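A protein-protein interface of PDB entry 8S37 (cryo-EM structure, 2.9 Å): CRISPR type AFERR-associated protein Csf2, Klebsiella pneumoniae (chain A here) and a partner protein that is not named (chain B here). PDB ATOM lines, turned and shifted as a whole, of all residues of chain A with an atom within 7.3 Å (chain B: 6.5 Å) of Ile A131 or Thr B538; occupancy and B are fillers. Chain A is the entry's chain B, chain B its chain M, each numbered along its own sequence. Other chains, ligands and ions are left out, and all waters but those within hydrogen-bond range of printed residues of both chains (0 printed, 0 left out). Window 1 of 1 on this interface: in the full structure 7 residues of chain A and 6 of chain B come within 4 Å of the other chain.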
ATOM      1  N   GLY A   8     -28.286   9.620  27.131  1.00  0.00           N
ATOM      2  CA  GLY A   8     -28.523  10.540  28.220  1.00  0.00           C
ATOM      3  C   GLY A   8     -28.087  11.945  27.895  1.00  0.00           C
ATOM      4  O   GLY A   8     -27.747  12.265  26.756  1.00  0.00           O
ATOM      5  N   ILE A  10     -25.832  15.409  29.397  1.00  0.00           N
ATOM      6  CA  ILE A  10     -24.794  15.989  30.235  1.00  0.00           C
ATOM      7  C   ILE A  10     -25.172  17.453  30.425  1.00  0.00           C
ATOM      8  O   ILE A  10     -24.954  18.279  29.530  1.00  0.00           O
ATOM      9  CB  ILE A  10     -23.404  15.836  29.608  1.00  0.00           C
ATOM     10  CG1 ILE A  10     -23.151  14.369  29.246  1.00  0.00           C
ATOM     11  CG2 ILE A  10     -22.315  16.330  30.553  1.00  0.00           C
ATOM     12  CD1 ILE A  10     -21.759  14.087  28.729  1.00  0.00           C
ATOM     13  N   ASN A  34     -19.103  20.694  14.588  1.00  0.00           N
ATOM     14  CA  ASN A  34     -19.848  19.623  13.931  1.00  0.00           C
ATOM     15  C   ASN A  34     -19.856  19.876  12.423  1.00  0.00           C
ATOM     16  O   ASN A  34     -20.876  20.187  11.807  1.00  0.00           O
ATOM     17  CB  ASN A  34     -21.255  19.545  14.508  1.00  0.00           C
ATOM     18  CG  ASN A  34     -21.929  18.220  14.239  1.00  0.00           C
ATOM     19  OD1 ASN A  34     -21.295  17.168  14.269  1.00  0.00           O
ATOM     20  ND2 ASN A  34     -23.230  18.263  13.986  1.00  0.00           N
ATOM     21  N   ALA A  40     -22.583  23.678  14.897  1.00  0.00           N
ATOM     22  CA  ALA A  40     -22.708  23.561  16.341  1.00  0.00           C
ATOM     23  C   ALA A  40     -21.430  22.952  16.909  1.00  0.00           C
ATOM     24  O   ALA A  40     -21.051  21.853  16.490  1.00  0.00           O
ATOM     25  CB  ALA A  40     -23.909  22.697  16.701  1.00  0.00           C
ATOM     26  N   PRO A  41     -20.732  23.606  17.839  1.00  0.00           N
ATOM     27  CA  PRO A  41     -19.604  22.936  18.491  1.00  0.00           C
ATOM     28  C   PRO A  41     -20.061  21.746  19.314  1.00  0.00           C
ATOM     29  O   PRO A  41     -21.140  21.749  19.910  1.00  0.00           O
ATOM     30  CB  PRO A  41     -18.991  24.030  19.373  1.00  0.00           C
ATOM     31  CG  PRO A  41     -20.022  25.074  19.479  1.00  0.00           C
ATOM     32  CD  PRO A  41     -20.760  25.036  18.188  1.00  0.00           C
ATOM     33  N   TYR A  42     -19.221  20.717  19.332  1.00  0.00           N
ATOM     34  CA  TYR A  42     -19.477  19.486  20.060  1.00  0.00           C
ATOM     35  C   TYR A  42     -18.291  19.193  20.959  1.00  0.00           C
ATOM     36  O   TYR A  42     -17.144  19.443  20.582  1.00  0.00           O
ATOM     37  CB  TYR A  42     -19.692  18.311  19.108  1.00  0.00           C
ATOM     38  CG  TYR A  42     -18.429  17.879  18.401  1.00  0.00           C
ATOM     39  CD1 TYR A  42     -17.962  18.566  17.292  1.00  0.00           C
ATOM     40  CD2 TYR A  42     -17.700  16.787  18.848  1.00  0.00           C
ATOM     41  CE1 TYR A  42     -16.807  18.178  16.649  1.00  0.00           C
ATOM     42  CE2 TYR A  42     -16.545  16.393  18.210  1.00  0.00           C
ATOM     43  CZ  TYR A  42     -16.103  17.092  17.112  1.00  0.00           C
ATOM     44  OH  TYR A  42     -14.952  16.699  16.474  1.00  0.00           O
ATOM     45  N   PHE A  43     -18.563  18.668  22.143  1.00  0.00           N
ATOM     46  CA  PHE A  43     -17.484  18.209  23.000  1.00  0.00           C
ATOM     47  C   PHE A  43     -16.985  16.867  22.475  1.00  0.00           C
ATOM     48  O   PHE A  43     -17.791  15.942  22.328  1.00  0.00           O
ATOM     49  CB  PHE A  43     -17.939  18.068  24.438  1.00  0.00           C
ATOM     50  CG  PHE A  43     -16.807  17.897  25.398  1.00  0.00           C
ATOM     51  CD1 PHE A  43     -15.988  18.962  25.713  1.00  0.00           C
ATOM     52  CD2 PHE A  43     -16.545  16.671  25.969  1.00  0.00           C
ATOM     53  CE1 PHE A  43     -14.941  18.812  26.588  1.00  0.00           C
ATOM     54  CE2 PHE A  43     -15.497  16.513  26.845  1.00  0.00           C
ATOM     55  CZ  PHE A  43     -14.692  17.587  27.153  1.00  0.00           C
ATOM     56  N   ILE A  48     -14.098  12.758  26.510  1.00  0.00           N
ATOM     57  CA  ILE A  48     -14.932  12.014  27.448  1.00  0.00           C
ATOM     58  C   ILE A  48     -14.391  10.602  27.607  1.00  0.00           C
ATOM     59  O   ILE A  48     -14.321  10.067  28.719  1.00  0.00           O
ATOM     60  CB  ILE A  48     -16.405  12.005  26.990  1.00  0.00           C
ATOM     61  CG1 ILE A  48     -16.921  13.425  26.724  1.00  0.00           C
ATOM     62  CG2 ILE A  48     -17.291  11.335  28.047  1.00  0.00           C
ATOM     63  CD1 ILE A  48     -18.314  13.472  26.114  1.00  0.00           C
ATOM     64  N   GLY A 128     -19.466   8.336  22.553  1.00  0.00           N
ATOM     65  CA  GLY A 128     -19.776   9.253  21.480  1.00  0.00           C
ATOM     66  C   GLY A 128     -19.608  10.704  21.867  1.00  0.00           C
ATOM     67  O   GLY A 128     -19.452  11.061  23.032  1.00  0.00           O
ATOM     68  N   ASN A 129     -19.616  11.552  20.844  1.00  0.00           N
ATOM     69  CA  ASN A 129     -19.540  12.988  21.056  1.00  0.00           C
ATOM     70  C   ASN A 129     -20.779  13.491  21.783  1.00  0.00           C
ATOM     71  O   ASN A 129     -21.885  12.972  21.611  1.00  0.00           O
ATOM     72  CB  ASN A 129     -19.391  13.715  19.724  1.00  0.00           C
ATOM     73  CG  ASN A 129     -18.123  13.333  18.997  1.00  0.00           C
ATOM     74  OD1 ASN A 129     -17.214  12.747  19.581  1.00  0.00           O
ATOM     75  ND2 ASN A 129     -18.053  13.668  17.718  1.00  0.00           N
ATOM     76  N   ALA A 130     -20.583  14.517  22.602  1.00  0.00           N
ATOM     77  CA  ALA A 130     -21.664  15.177  23.321  1.00  0.00           C
ATOM     78  C   ALA A 130     -22.072  16.410  22.525  1.00  0.00           C
ATOM     79  O   ALA A 130     -21.361  17.420  22.527  1.00  0.00           O
ATOM     80  CB  ALA A 130     -21.230  15.549  24.736  1.00  0.00           C
ATOM     81  N   ILE A 131     -23.213  16.328  21.850  1.00  0.00           N
ATOM     82  CA  ILE A 131     -23.689  17.408  20.990  1.00  0.00           C
ATOM     83  C   ILE A 131     -24.601  18.295  21.830  1.00  0.00           C
ATOM     84  O   ILE A 131     -25.327  17.768  22.683  1.00  0.00           O
ATOM     85  CB  ILE A 131     -24.439  16.873  19.758  1.00  0.00           C
ATOM     86  CG1 ILE A 131     -23.649  15.771  19.040  1.00  0.00           C
ATOM     87  CG2 ILE A 131     -24.746  18.011  18.795  1.00  0.00           C
ATOM     88  CD1 ILE A 131     -22.381  16.239  18.361  1.00  0.00           C
ATOM     89  N   PRO A 132     -24.634  19.611  21.634  1.00  0.00           N
ATOM     90  CA  PRO A 132     -25.481  20.452  22.483  1.00  0.00           C
ATOM     91  C   PRO A 132     -26.947  20.347  22.085  1.00  0.00           C
ATOM     92  O   PRO A 132     -27.304  19.828  21.027  1.00  0.00           O
ATOM     93  CB  PRO A 132     -24.957  21.872  22.237  1.00  0.00           C
ATOM     94  CG  PRO A 132     -23.689  21.710  21.512  1.00  0.00           C
ATOM     95  CD  PRO A 132     -23.798  20.443  20.753  1.00  0.00           C
ATOM     96  N   ASP A 133     -27.796  20.858  22.970  1.00  0.00           N
ATOM     97  CA  ASP A 133     -29.240  20.886  22.776  1.00  0.00           C
ATOM     98  C   ASP A 133     -29.667  22.336  22.623  1.00  0.00           C
ATOM     99  O   ASP A 133     -29.471  23.140  23.541  1.00  0.00           O
ATOM    100  CB  ASP A 133     -29.957  20.239  23.960  1.00  0.00           C
ATOM    101  CG  ASP A 133     -29.428  18.857  24.281  1.00  0.00           C
ATOM    102  OD1 ASP A 133     -28.553  18.364  23.538  1.00  0.00           O
ATOM    103  OD2 ASP A 133     -29.889  18.261  25.277  1.00  0.00           O
ATOM    104  N   GLY A 134     -30.241  22.670  21.478  1.00  0.00           N
ATOM    105  CA  GLY A 134     -30.685  24.043  21.289  1.00  0.00           C
ATOM    106  C   GLY A 134     -29.585  24.935  20.753  1.00  0.00           C
ATOM    107  O   GLY A 134     -28.394  24.698  20.952  1.00  0.00           O
ATOM    108  N   GLN A 137     -25.739  28.233  23.483  1.00  0.00           N
ATOM    109  CA  GLN A 137     -25.189  27.345  24.508  1.00  0.00           C
ATOM    110  C   GLN A 137     -23.675  27.225  24.407  1.00  0.00           C
ATOM    111  O   GLN A 137     -23.094  26.373  25.090  1.00  0.00           O
ATOM    112  CB  GLN A 137     -25.788  25.935  24.494  1.00  0.00           C
ATOM    113  CG  GLN A 137     -27.301  25.916  24.507  1.00  0.00           C
ATOM    114  CD  GLN A 137     -27.856  24.781  25.340  1.00  0.00           C
ATOM    115  OE1 GLN A 137     -27.235  23.726  25.467  1.00  0.00           O
ATOM    116  NE2 GLN A 137     -29.032  24.994  25.917  1.00  0.00           N
ATOM    117  N   PHE A 242     -18.898  25.504  26.235  1.00  0.00           N
ATOM    118  CA  PHE A 242     -20.337  25.345  26.390  1.00  0.00           C
ATOM    119  C   PHE A 242     -20.784  26.006  27.684  1.00  0.00           C
ATOM    120  O   PHE A 242     -20.179  25.791  28.737  1.00  0.00           O
ATOM    121  CB  PHE A 242     -20.722  23.869  26.385  1.00  0.00           C
ATOM    122  CG  PHE A 242     -20.267  23.139  25.165  1.00  0.00           C
ATOM    123  CD1 PHE A 242     -20.902  23.335  23.955  1.00  0.00           C
ATOM    124  CD2 PHE A 242     -19.204  22.261  25.222  1.00  0.00           C
ATOM    125  CE1 PHE A 242     -20.483  22.672  22.826  1.00  0.00           C
ATOM    126  CE2 PHE A 242     -18.783  21.592  24.094  1.00  0.00           C
ATOM    127  CZ  PHE A 242     -19.427  21.796  22.896  1.00  0.00           C
ATOM    128  N   GLU A 247     -27.183  21.760  28.031  1.00  0.00           N
ATOM    129  CA  GLU A 247     -27.607  20.373  27.898  1.00  0.00           C
ATOM    130  C   GLU A 247     -26.933  19.781  26.669  1.00  0.00           C
ATOM    131  O   GLU A 247     -27.140  20.272  25.554  1.00  0.00           O
ATOM    132  CB  GLU A 247     -29.127  20.278  27.771  1.00  0.00           C
ATOM    133  CG  GLU A 247     -29.896  20.768  28.987  1.00  0.00           C
ATOM    134  CD  GLU A 247     -29.830  19.801  30.150  1.00  0.00           C
ATOM    135  OE1 GLU A 247     -29.149  18.762  30.026  1.00  0.00           O
ATOM    136  OE2 GLU A 247     -30.463  20.079  31.190  1.00  0.00           O
ATOM    137  N   LEU A 248     -26.128  18.737  26.866  1.00  0.00           N
ATOM    138  CA  LEU A 248     -25.404  18.090  25.777  1.00  0.00           C
ATOM    139  C   LEU A 248     -25.857  16.640  25.680  1.00  0.00           C
ATOM    140  O   LEU A 248     -25.582  15.839  26.577  1.00  0.00           O
ATOM    141  CB  LEU A 248     -23.895  18.175  25.988  1.00  0.00           C
ATOM    142  CG  LEU A 248     -23.281  19.572  25.882  1.00  0.00           C
ATOM    143  CD1 LEU A 248     -23.416  20.348  27.183  1.00  0.00           C
ATOM    144  CD2 LEU A 248     -21.824  19.475  25.465  1.00  0.00           C
ATOM    145  N   SER A 249     -26.564  16.305  24.605  1.00  0.00           N
ATOM    146  CA  SER A 249     -27.013  14.934  24.411  1.00  0.00           C
ATOM    147  C   SER A 249     -25.814  14.036  24.130  1.00  0.00           C
ATOM    148  O   SER A 249     -24.973  14.355  23.284  1.00  0.00           O
ATOM    149  CB  SER A 249     -28.015  14.860  23.263  1.00  0.00           C
ATOM    150  OG  SER A 249     -27.439  15.332  22.058  1.00  0.00           O
ATOM    151  N   HIS A 250     -25.738  12.917  24.845  1.00  0.00           N
ATOM    152  CA  HIS A 250     -24.593  12.023  24.818  1.00  0.00           C
ATOM    153  C   HIS A 250     -25.064  10.586  24.664  1.00  0.00           C
ATOM    154  O   HIS A 250     -26.040  10.167  25.300  1.00  0.00           O
ATOM    155  CB  HIS A 250     -23.768  12.167  26.094  1.00  0.00           C
ATOM    156  CG  HIS A 250     -22.377  11.637  25.975  1.00  0.00           C
ATOM    157  ND1 HIS A 250     -21.851  10.719  26.857  1.00  0.00           N
ATOM    158  CD2 HIS A 250     -21.401  11.902  25.078  1.00  0.00           C
ATOM    159  CE1 HIS A 250     -20.608  10.440  26.507  1.00  0.00           C
ATOM    160  NE2 HIS A 250     -20.312  11.142  25.428  1.00  0.00           N
ATOM    161  N   ARG A 251     -24.373   9.835  23.810  1.00  0.00           N
ATOM    162  CA  ARG A 251     -24.658   8.423  23.599  1.00  0.00           C
ATOM    163  C   ARG A 251     -23.373   7.624  23.736  1.00  0.00           C
ATOM    164  O   ARG A 251     -22.363   7.950  23.106  1.00  0.00           O
ATOM    165  CB  ARG A 251     -25.287   8.189  22.225  1.00  0.00           C
ATOM    166  CG  ARG A 251     -26.654   8.823  22.077  1.00  0.00           C
ATOM    167  CD  ARG A 251     -27.299   8.483  20.748  1.00  0.00           C
ATOM    168  NE  ARG A 251     -28.750   8.592  20.821  1.00  0.00           N
ATOM    169  CZ  ARG A 251     -29.547   7.674  21.353  1.00  0.00           C
ATOM    170  NH1 ARG A 251     -29.070   6.552  21.868  1.00  0.00           N
ATOM    171  NH2 ARG A 251     -30.859   7.888  21.371  1.00  0.00           N
ATOM    172  N   TYR B 527     -37.130  20.808  17.811  1.00  0.00           N
ATOM    173  CA  TYR B 527     -36.126  19.956  18.432  1.00  0.00           C
ATOM    174  C   TYR B 527     -36.555  19.556  19.834  1.00  0.00           C
ATOM    175  O   TYR B 527     -36.359  18.410  20.244  1.00  0.00           O
ATOM    176  CB  TYR B 527     -34.773  20.665  18.455  1.00  0.00           C
ATOM    177  CG  TYR B 527     -33.752  19.974  19.317  1.00  0.00           C
ATOM    178  CD1 TYR B 527     -33.305  18.698  19.008  1.00  0.00           C
ATOM    179  CD2 TYR B 527     -33.230  20.596  20.439  1.00  0.00           C
ATOM    180  CE1 TYR B 527     -32.371  18.061  19.794  1.00  0.00           C
ATOM    181  CE2 TYR B 527     -32.297  19.968  21.230  1.00  0.00           C
ATOM    182  CZ  TYR B 527     -31.870  18.699  20.904  1.00  0.00           C
ATOM    183  OH  TYR B 527     -30.938  18.064  21.688  1.00  0.00           O
ATOM    184  N   SER B 536     -34.265  10.990  18.723  1.00  0.00           N
ATOM    185  CA  SER B 536     -32.909  11.513  18.874  1.00  0.00           C
ATOM    186  C   SER B 536     -32.433  12.058  17.531  1.00  0.00           C
ATOM    187  O   SER B 536     -31.893  11.326  16.702  1.00  0.00           O
ATOM    188  CB  SER B 536     -31.972  10.430  19.394  1.00  0.00           C
ATOM    189  OG  SER B 536     -32.396   9.956  20.660  1.00  0.00           O
ATOM    190  N   ARG B 537     -32.641  13.354  17.311  1.00  0.00           N
ATOM    191  CA  ARG B 537     -31.941  14.066  16.253  1.00  0.00           C
ATOM    192  C   ARG B 537     -31.451  15.397  16.803  1.00  0.00           C
ATOM    193  O   ARG B 537     -32.181  16.091  17.515  1.00  0.00           O
ATOM    194  CB  ARG B 537     -32.815  14.265  15.002  1.00  0.00           C
ATOM    195  CG  ARG B 537     -33.938  15.286  15.096  1.00  0.00           C
ATOM    196  CD  ARG B 537     -34.575  15.488  13.724  1.00  0.00           C
ATOM    197  NE  ARG B 537     -35.306  14.309  13.268  1.00  0.00           N
ATOM    198  CZ  ARG B 537     -34.805  13.335  12.517  1.00  0.00           C
ATOM    199  NH1 ARG B 537     -33.546  13.345  12.105  1.00  0.00           N
ATOM    200  NH2 ARG B 537     -35.589  12.319  12.169  1.00  0.00           N
ATOM    201  N   THR B 538     -30.218  15.744  16.457  1.00  0.00           N
ATOM    202  CA  THR B 538     -29.582  16.938  16.986  1.00  0.00           C
ATOM    203  C   THR B 538     -30.252  18.194  16.445  1.00  0.00           C
ATOM    204  O   THR B 538     -30.999  18.165  15.465  1.00  0.00           O
ATOM    205  CB  THR B 538     -28.095  16.956  16.643  1.00  0.00           C
ATOM    206  OG1 THR B 538     -27.914  16.588  15.270  1.00  0.00           O
ATOM    207  CG2 THR B 538     -27.340  15.992  17.537  1.00  0.00           C
ATOM    208  N   PHE B 539     -29.978  19.314  17.117  1.00  0.00           N
ATOM    209  CA  PHE B 539     -30.653  20.562  16.782  1.00  0.00           C
ATOM    210  C   PHE B 539     -30.333  20.998  15.359  1.00  0.00           C
ATOM    211  O   PHE B 539     -31.201  21.532  14.661  1.00  0.00           O
ATOM    212  CB  PHE B 539     -30.262  21.660  17.767  1.00  0.00           C
ATOM    213  CG  PHE B 539     -30.628  23.032  17.298  1.00  0.00           C
ATOM    214  CD1 PHE B 539     -31.946  23.454  17.322  1.00  0.00           C
ATOM    215  CD2 PHE B 539     -29.662  23.896  16.815  1.00  0.00           C
ATOM    216  CE1 PHE B 539     -32.292  24.713  16.882  1.00  0.00           C
ATOM    217  CE2 PHE B 539     -30.003  25.158  16.374  1.00  0.00           C
ATOM    218  CZ  PHE B 539     -31.320  25.564  16.405  1.00  0.00           C
ATOM    219  N   GLU B 540     -29.089  20.810  14.918  1.00  0.00           N
ATOM    220  CA  GLU B 540     -28.743  21.166  13.546  1.00  0.00           C
ATOM    221  C   GLU B 540     -29.534  20.337  12.543  1.00  0.00           C
ATOM    222  O   GLU B 540     -29.876  20.829  11.462  1.00  0.00           O
ATOM    223  CB  GLU B 540     -27.243  20.985  13.317  1.00  0.00           C
ATOM    224  CG  GLU B 540     -26.371  21.902  14.160  1.00  0.00           C
ATOM    225  CD  GLU B 540     -26.546  23.366  13.804  1.00  0.00           C
ATOM    226  OE1 GLU B 540     -27.115  23.654  12.731  1.00  0.00           O
ATOM    227  OE2 GLU B 540     -26.118  24.228  14.600  1.00  0.00           O
ATOM    228  N   ALA B 541     -29.845  19.086  12.883  1.00  0.00           N
ATOM    229  CA  ALA B 541     -30.701  18.285  12.014  1.00  0.00           C
ATOM    230  C   ALA B 541     -32.086  18.907  11.893  1.00  0.00           C
ATOM    231  O   ALA B 541     -32.662  18.950  10.800  1.00  0.00           O
ATOM    232  CB  ALA B 541     -30.797  16.854  12.541  1.00  0.00           C
ATOM    233  N   VAL B 542     -32.644  19.379  13.009  1.00  0.00           N
ATOM    234  CA  VAL B 542     -33.953  20.021  12.957  1.00  0.00           C
ATOM    235  C   VAL B 542     -33.867  21.329  12.182  1.00  0.00           C
ATOM    236  O   VAL B 542     -34.803  21.705  11.469  1.00  0.00           O
ATOM    237  CB  VAL B 542     -34.495  20.245  14.380  1.00  0.00           C
ATOM    238  CG1 VAL B 542     -35.939  20.730  14.333  1.00  0.00           C
ATOM    239  CG2 VAL B 542     -34.378  18.969  15.196  1.00  0.00           C
ATOM    240  N   ASN B 543     -32.745  22.037  12.309  1.00  0.00           N
ATOM    241  CA  ASN B 543     -32.524  23.234  11.504  1.00  0.00           C
ATOM    242  C   ASN B 543     -32.565  22.898  10.022  1.00  0.00           C
ATOM    243  O   ASN B 543     -33.198  23.605   9.232  1.00  0.00           O
ATOM    244  CB  ASN B 543     -31.183  23.876  11.866  1.00  0.00           C
ATOM    245  CG  ASN B 543     -31.312  25.338  12.252  1.00  0.00           C
ATOM    246  OD1 ASN B 543     -32.303  25.754  12.849  1.00  0.00           O
ATOM    247  ND2 ASN B 543     -30.300  26.126  11.914  1.00  0.00           N
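The side-chain carboxylate (OD1) of Asp A133 lies within hydrogen-bond range of the backbone NH (N) of Ser A249, at 3.1 Å.
The backbone NH of Asn A34 is in hydrogen-bond range of the backbone carbonyl oxygen of Ala A40.
O of Asp A133 lies close to OE1 of Gln A137, at 3.0 Å.
O of Arg A251 is in hydrogen-bond range of N of Gly A128 (3.0 Å).
The backbone carbonyl oxygen (O) of Ile A131 sits at hydrogen-bond distance from the backbone NH (N) of Ser A249, 2.7 Å away.
The backbone NH of Asp A133 sits at hydrogen-bond distance from the backbone carbonyl oxygen of Glu A247, at 2.7 Å.
Of chain B, only Thr B538 comes within 4 Å of Ile A131.
Printed residues of chain A within 4 Å of Thr B538: Ile A131.
Of the printed residues of chain A, Glu B540 touches Ala A40 (3.4 Å).
Printed residues of chain B within 4 Å of Ala A40: Glu B540.
Ile A48 touches none of the printed residues of chain B.
Phe A242 touches none of the printed residues of chain B.
The nearest residue of chain A that does not touch Thr B538 is Ser A249 (4.6 Å).
The side-chain hydroxyl of Tyr B527 is in hydrogen-bond range of the side-chain carboxylate of Asp A133 (3.0 Å).
The side-chain hydroxyl (OG) of Ser B536 lies within hydrogen-bond range of the guanidinium group (NH2) of Arg A251, 2.7 Å away.
Glu B540 touches Ala A40.
Thr B538 touches Ile A131 (CG2 to CG2, 3.5 Å).
N of Gly A134 touches CE2 of Tyr B527, 3.4 Å away.
Gly A134 touches Phe B539.
Of the 9 printed residues of chain B, 5 touch a printed residue of chain A.
Hydrophobic or aromatic side chains of chain B within 4 Å of the printed part of chain A: Tyr B527 and Phe B539.
Hydrophobic or aromatic side chains of chain A within 4 Å of the printed part of chain B: Ala A40 and Ile A131.
Among the printed residues, no Asp or Glu carboxylate lies within 4 Å of a Lys or Arg side-chain nitrogen of the other chain.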
